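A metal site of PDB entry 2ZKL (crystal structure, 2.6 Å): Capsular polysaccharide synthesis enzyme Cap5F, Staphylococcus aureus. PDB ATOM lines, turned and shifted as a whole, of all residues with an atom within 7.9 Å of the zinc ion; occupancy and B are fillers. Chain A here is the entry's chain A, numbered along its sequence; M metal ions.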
ATOM      1  N   GLY A 286      30.977 -27.482  28.902  1.00  0.00           N
ATOM      2  CA  GLY A 286      30.148 -27.715  27.746  1.00  0.00           C
ATOM      3  C   GLY A 286      29.160 -28.848  27.878  1.00  0.00           C
ATOM      4  O   GLY A 286      28.305 -28.844  28.761  1.00  0.00           O
ATOM      5  N   ASN A 287      29.301 -29.834  26.991  1.00  0.00           N
ATOM      6  CA  ASN A 287      28.407 -30.993  26.950  1.00  0.00           C
ATOM      7  C   ASN A 287      26.976 -30.513  26.731  1.00  0.00           C
ATOM      8  O   ASN A 287      26.071 -30.811  27.526  1.00  0.00           O
ATOM      9  CB  ASN A 287      28.496 -31.814  28.255  1.00  0.00           C
ATOM     10  CG  ASN A 287      29.772 -32.640  28.354  1.00  0.00           C
ATOM     11  OD1 ASN A 287      30.111 -33.396  27.435  1.00  0.00           O
ATOM     12  ND2 ASN A 287      30.470 -32.515  29.473  1.00  0.00           N
ATOM     13  N   HIS A 288      26.779 -29.755  25.653  1.00  0.00           N
ATOM     14  CA  HIS A 288      25.467 -29.223  25.294  1.00  0.00           C
ATOM     15  C   HIS A 288      25.448 -28.880  23.804  1.00  0.00           C
ATOM     16  O   HIS A 288      26.502 -28.815  23.184  1.00  0.00           O
ATOM     17  CB  HIS A 288      25.134 -27.985  26.146  1.00  0.00           C
ATOM     18  CG  HIS A 288      26.134 -26.863  26.041  1.00  0.00           C
ATOM     19  ND1 HIS A 288      26.383 -25.998  27.082  1.00  0.00           N
ATOM     20  CD2 HIS A 288      26.922 -26.455  25.016  1.00  0.00           C
ATOM     21  CE1 HIS A 288      27.271 -25.090  26.701  1.00  0.00           C
ATOM     22  NE2 HIS A 288      27.607 -25.352  25.448  1.00  0.00           N
ATOM     23  N   TRP A 289      24.256 -28.726  23.228  1.00  0.00           N
ATOM     24  CA  TRP A 289      24.147 -28.345  21.827  1.00  0.00           C
ATOM     25  C   TRP A 289      23.210 -27.152  21.656  1.00  0.00           C
ATOM     26  O   TRP A 289      22.554 -26.730  22.611  1.00  0.00           O
ATOM     27  CB  TRP A 289      23.674 -29.510  20.954  1.00  0.00           C
ATOM     28  CG  TRP A 289      22.351 -30.109  21.343  1.00  0.00           C
ATOM     29  CD1 TRP A 289      22.129 -31.019  22.342  1.00  0.00           C
ATOM     30  CD2 TRP A 289      21.075 -29.868  20.727  1.00  0.00           C
ATOM     31  NE1 TRP A 289      20.799 -31.356  22.385  1.00  0.00           N
ATOM     32  CE2 TRP A 289      20.123 -30.663  21.411  1.00  0.00           C
ATOM     33  CE3 TRP A 289      20.642 -29.046  19.670  1.00  0.00           C
ATOM     34  CZ2 TRP A 289      18.766 -30.672  21.063  1.00  0.00           C
ATOM     35  CZ3 TRP A 289      19.292 -29.052  19.334  1.00  0.00           C
ATOM     36  CH2 TRP A 289      18.368 -29.864  20.023  1.00  0.00           C
ATOM     37  N   HIS A 290      23.184 -26.601  20.442  1.00  0.00           N
ATOM     38  CA  HIS A 290      22.338 -25.450  20.159  1.00  0.00           C
ATOM     39  C   HIS A 290      21.578 -25.670  18.874  1.00  0.00           C
ATOM     40  O   HIS A 290      21.992 -26.463  18.029  1.00  0.00           O
ATOM     41  CB  HIS A 290      23.184 -24.199  19.994  1.00  0.00           C
ATOM     42  CG  HIS A 290      24.261 -24.037  21.019  1.00  0.00           C
ATOM     43  ND1 HIS A 290      24.007 -23.597  22.303  1.00  0.00           N
ATOM     44  CD2 HIS A 290      25.597 -24.222  20.939  1.00  0.00           C
ATOM     45  CE1 HIS A 290      25.150 -23.524  22.970  1.00  0.00           C
ATOM     46  NE2 HIS A 290      26.125 -23.903  22.162  1.00  0.00           N
ATOM     47  N   LYS A 293      22.494 -21.145  17.815  1.00  0.00           N
ATOM     48  CA  LYS A 293      23.607 -20.441  18.426  1.00  0.00           C
ATOM     49  C   LYS A 293      24.805 -21.237  17.925  1.00  0.00           C
ATOM     50  O   LYS A 293      24.747 -22.466  17.872  1.00  0.00           O
ATOM     51  CB  LYS A 293      23.558 -20.539  19.955  1.00  0.00           C
ATOM     52  CG  LYS A 293      24.739 -19.823  20.617  1.00  0.00           C
ATOM     53  CD  LYS A 293      24.863 -20.088  22.115  1.00  0.00           C
ATOM     54  CE  LYS A 293      23.592 -19.753  22.910  1.00  0.00           C
ATOM     55  NZ  LYS A 293      23.118 -18.340  22.805  1.00  0.00           N
ATOM     56  N   ASN A 294      25.872 -20.551  17.529  1.00  0.00           N
ATOM     57  CA  ASN A 294      27.080 -21.232  17.096  1.00  0.00           C
ATOM     58  C   ASN A 294      28.293 -20.414  17.498  1.00  0.00           C
ATOM     59  O   ASN A 294      28.218 -19.194  17.672  1.00  0.00           O
ATOM     60  CB  ASN A 294      27.081 -21.520  15.586  1.00  0.00           C
ATOM     61  CG  ASN A 294      27.195 -20.283  14.728  1.00  0.00           C
ATOM     62  OD1 ASN A 294      26.197 -19.698  14.314  1.00  0.00           O
ATOM     63  ND2 ASN A 294      28.422 -19.877  14.456  1.00  0.00           N
ATOM     64  N   GLU A 295      29.417 -21.096  17.655  1.00  0.00           N
ATOM     65  CA  GLU A 295      30.615 -20.415  18.104  1.00  0.00           C
ATOM     66  C   GLU A 295      31.885 -20.686  17.329  1.00  0.00           C
ATOM     67  O   GLU A 295      31.922 -21.480  16.374  1.00  0.00           O
ATOM     68  CB  GLU A 295      30.834 -20.760  19.561  1.00  0.00           C
ATOM     69  CG  GLU A 295      29.564 -20.607  20.362  1.00  0.00           C
ATOM     70  CD  GLU A 295      29.399 -21.708  21.381  1.00  0.00           C
ATOM     71  OE1 GLU A 295      29.045 -22.848  20.976  1.00  0.00           O
ATOM     72  OE2 GLU A 295      29.625 -21.436  22.579  1.00  0.00           O
ATOM     73  N   LYS A 296      32.936 -20.000  17.748  1.00  0.00           N
ATOM     74  CA  LYS A 296      34.265 -20.141  17.190  1.00  0.00           C
ATOM     75  C   LYS A 296      35.194 -20.186  18.403  1.00  0.00           C
ATOM     76  O   LYS A 296      35.300 -19.201  19.127  1.00  0.00           O
ATOM     77  CB  LYS A 296      34.622 -18.946  16.303  1.00  0.00           C
ATOM     78  CG  LYS A 296      34.129 -19.040  14.865  1.00  0.00           C
ATOM     79  CD  LYS A 296      34.435 -17.727  14.142  1.00  0.00           C
ATOM     80  CE  LYS A 296      33.847 -17.659  12.743  1.00  0.00           C
ATOM     81  NZ  LYS A 296      34.300 -18.767  11.890  1.00  0.00           N
ATOM     82  N   PHE A 297      35.830 -21.324  18.632  1.00  0.00           N
ATOM     83  CA  PHE A 297      36.749 -21.482  19.760  1.00  0.00           C
ATOM     84  C   PHE A 297      38.199 -21.310  19.282  1.00  0.00           C
ATOM     85  O   PHE A 297      38.577 -21.850  18.247  1.00  0.00           O
ATOM     86  CB  PHE A 297      36.626 -22.875  20.388  1.00  0.00           C
ATOM     87  CG  PHE A 297      35.378 -23.076  21.221  1.00  0.00           C
ATOM     88  CD1 PHE A 297      34.442 -22.064  21.383  1.00  0.00           C
ATOM     89  CD2 PHE A 297      35.161 -24.302  21.855  1.00  0.00           C
ATOM     90  CE1 PHE A 297      33.311 -22.265  22.163  1.00  0.00           C
ATOM     91  CE2 PHE A 297      34.023 -24.515  22.633  1.00  0.00           C
ATOM     92  CZ  PHE A 297      33.094 -23.491  22.796  1.00  0.00           C
ATOM     93  N   ILE A 331      31.906 -24.316  15.858  1.00  0.00           N
ATOM     94  CA  ILE A 331      31.030 -25.221  16.607  1.00  0.00           C
ATOM     95  C   ILE A 331      29.736 -25.270  15.803  1.00  0.00           C
ATOM     96  O   ILE A 331      28.887 -24.404  15.950  1.00  0.00           O
ATOM     97  CB  ILE A 331      30.720 -24.668  18.003  1.00  0.00           C
ATOM     98  CG1 ILE A 331      32.030 -24.216  18.678  1.00  0.00           C
ATOM     99  CG2 ILE A 331      30.018 -25.716  18.829  1.00  0.00           C
ATOM    100  CD1 ILE A 331      33.072 -25.321  18.848  1.00  0.00           C
ATOM    101  N   PRO A 332      29.587 -26.265  14.925  1.00  0.00           N
ATOM    102  CA  PRO A 332      28.358 -26.357  14.112  1.00  0.00           C
ATOM    103  C   PRO A 332      27.141 -26.706  14.945  1.00  0.00           C
ATOM    104  O   PRO A 332      27.238 -27.493  15.887  1.00  0.00           O
ATOM    105  CB  PRO A 332      28.684 -27.460  13.097  1.00  0.00           C
ATOM    106  CG  PRO A 332      30.193 -27.470  13.058  1.00  0.00           C
ATOM    107  CD  PRO A 332      30.550 -27.292  14.501  1.00  0.00           C
ATOM    108  N   TYR A 335      25.388 -30.274  17.078  1.00  0.00           N
ATOM    109  CA  TYR A 335      26.367 -31.201  17.658  1.00  0.00           C
ATOM    110  C   TYR A 335      26.580 -30.830  19.118  1.00  0.00           C
ATOM    111  O   TYR A 335      26.818 -29.659  19.422  1.00  0.00           O
ATOM    112  CB  TYR A 335      27.723 -31.114  16.955  1.00  0.00           C
ATOM    113  CG  TYR A 335      27.772 -31.587  15.517  1.00  0.00           C
ATOM    114  CD1 TYR A 335      27.289 -30.797  14.476  1.00  0.00           C
ATOM    115  CD2 TYR A 335      28.314 -32.835  15.192  1.00  0.00           C
ATOM    116  CE1 TYR A 335      27.354 -31.229  13.143  1.00  0.00           C
ATOM    117  CE2 TYR A 335      28.372 -33.289  13.867  1.00  0.00           C
ATOM    118  CZ  TYR A 335      27.888 -32.476  12.847  1.00  0.00           C
ATOM    119  OH  TYR A 335      27.903 -32.909  11.540  1.00  0.00           O
ATOM    120  N   THR A 336      26.489 -31.787  20.042  1.00  0.00           N
ATOM    121  CA  THR A 336      26.804 -31.421  21.424  1.00  0.00           C
ATOM    122  C   THR A 336      28.314 -31.313  21.360  1.00  0.00           C
ATOM    123  O   THR A 336      28.959 -31.961  20.533  1.00  0.00           O
ATOM    124  CB  THR A 336      26.475 -32.490  22.457  1.00  0.00           C
ATOM    125  OG1 THR A 336      26.612 -33.798  21.879  1.00  0.00           O
ATOM    126  CG2 THR A 336      25.090 -32.288  22.991  1.00  0.00           C
ATOM    127  N   HIS A 337      28.876 -30.493  22.229  1.00  0.00           N
ATOM    128  CA  HIS A 337      30.304 -30.324  22.227  1.00  0.00           C
ATOM    129  C   HIS A 337      30.754 -30.010  23.615  1.00  0.00           C
ATOM    130  O   HIS A 337      29.962 -29.567  24.451  1.00  0.00           O
ATOM    131  CB  HIS A 337      30.677 -29.181  21.293  1.00  0.00           C
ATOM    132  CG  HIS A 337      29.823 -27.964  21.472  1.00  0.00           C
ATOM    133  ND1 HIS A 337      28.574 -27.845  20.901  1.00  0.00           N
ATOM    134  CD2 HIS A 337      30.006 -26.836  22.206  1.00  0.00           C
ATOM    135  CE1 HIS A 337      28.024 -26.706  21.271  1.00  0.00           C
ATOM    136  NE2 HIS A 337      28.867 -26.073  22.064  1.00  0.00           N
ATOM    137  N   ASN A 338      32.032 -30.256  23.881  1.00  0.00           N
ATOM    138  CA  ASN A 338      32.622 -29.931  25.160  1.00  0.00           C
ATOM    139  C   ASN A 338      34.109 -29.663  24.935  1.00  0.00           C
ATOM    140  O   ASN A 338      34.677 -30.040  23.911  1.00  0.00           O
ATOM    141  CB  ASN A 338      32.377 -31.042  26.214  1.00  0.00           C
ATOM    142  CG  ASN A 338      33.144 -32.342  25.945  1.00  0.00           C
ATOM    143  OD1 ASN A 338      32.821 -33.372  26.535  1.00  0.00           O
ATOM    144  ND2 ASN A 338      34.154 -32.304  25.069  1.00  0.00           N
ATOM    145  N   MET A 351      36.345 -17.195  22.805  1.00  0.00           N
ATOM    146  CA  MET A 351      35.116 -17.709  22.231  1.00  0.00           C
ATOM    147  C   MET A 351      34.289 -16.622  21.544  1.00  0.00           C
ATOM    148  O   MET A 351      33.905 -15.623  22.166  1.00  0.00           O
ATOM    149  CB  MET A 351      34.279 -18.402  23.329  1.00  0.00           C
ATOM    150  CG  MET A 351      34.895 -19.716  23.867  1.00  0.00           C
ATOM    151  SD  MET A 351      34.018 -20.575  25.233  1.00  0.00           S
ATOM    152  CE  MET A 351      32.323 -20.499  24.671  1.00  0.00           C
ATOM    153  N   VAL A 353      30.767 -15.820  19.640  1.00  0.00           N
ATOM    154  CA  VAL A 353      29.433 -16.400  19.519  1.00  0.00           C
ATOM    155  C   VAL A 353      28.588 -15.494  18.628  1.00  0.00           C
ATOM    156  O   VAL A 353      28.740 -14.280  18.642  1.00  0.00           O
ATOM    157  CB  VAL A 353      28.782 -16.597  20.915  1.00  0.00           C
ATOM    158  CG1 VAL A 353      28.543 -15.282  21.554  1.00  0.00           C
ATOM    159  CG2 VAL A 353      27.507 -17.398  20.785  1.00  0.00           C
ATOM    160  N   ASP A 363      19.589 -21.167  24.013  1.00  0.00           N
ATOM    161  CA  ASP A 363      19.479 -22.037  22.867  1.00  0.00           C
ATOM    162  C   ASP A 363      20.582 -23.037  23.088  1.00  0.00           C
ATOM    163  O   ASP A 363      21.383 -23.330  22.207  1.00  0.00           O
ATOM    164  CB  ASP A 363      19.696 -21.257  21.566  1.00  0.00           C
ATOM    165  CG  ASP A 363      19.653 -22.140  20.363  1.00  0.00           C
ATOM    166  OD1 ASP A 363      18.888 -23.121  20.385  1.00  0.00           O
ATOM    167  OD2 ASP A 363      20.354 -21.854  19.376  1.00  0.00           O
ATOM    168  N   THR A 364      20.622 -23.556  24.311  1.00  0.00           N
ATOM    169  CA  THR A 364      21.625 -24.532  24.693  1.00  0.00           C
ATOM    170  C   THR A 364      20.899 -25.647  25.458  1.00  0.00           C
ATOM    171  O   THR A 364      20.057 -25.383  26.310  1.00  0.00           O
ATOM    172  CB  THR A 364      22.734 -23.879  25.554  1.00  0.00           C
ATOM    173  OG1 THR A 364      22.345 -23.900  26.920  1.00  0.00           O
ATOM    174  CG2 THR A 364      22.945 -22.438  25.145  1.00  0.00           C
HETATM  175 ZN    ZN M   1      28.272 -23.923  22.734  1.00  0.00          ZN
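ND1 of His 290 is in hydrogen-bond range of O of Asp 363 (2.6 Å).
O of Glu 295 lies within hydrogen-bond range of N of Ile 331.
The backbone carbonyl oxygen of His 337 sits at hydrogen-bond distance from the backbone NH of Asn 287 (2.6 Å).
The backbone NH (N) of His 337 lies within hydrogen-bond range of the backbone carbonyl oxygen (O) of His 288 (3.1 Å).
ND1 of His 337 sits at hydrogen-bond distance from O of Tyr 335, at 2.9 Å.
Merely in contact with the zinc ion: His 288 (3.1 Å).
Within 4 Å of the zinc ion: His 288, His 290, Glu 295 and His 337.
OE1 of Glu 295 binds the zinc ion (2.2 Å).
The zinc ion is bound by a ring nitrogen (NE2) of His 290 (2.2 Å).
NE2 of His 337 is bound to the zinc ion, at 2.3 Å.
Slightly farther from the zinc ion lies OE2 of Glu 295 (2.8 Å).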
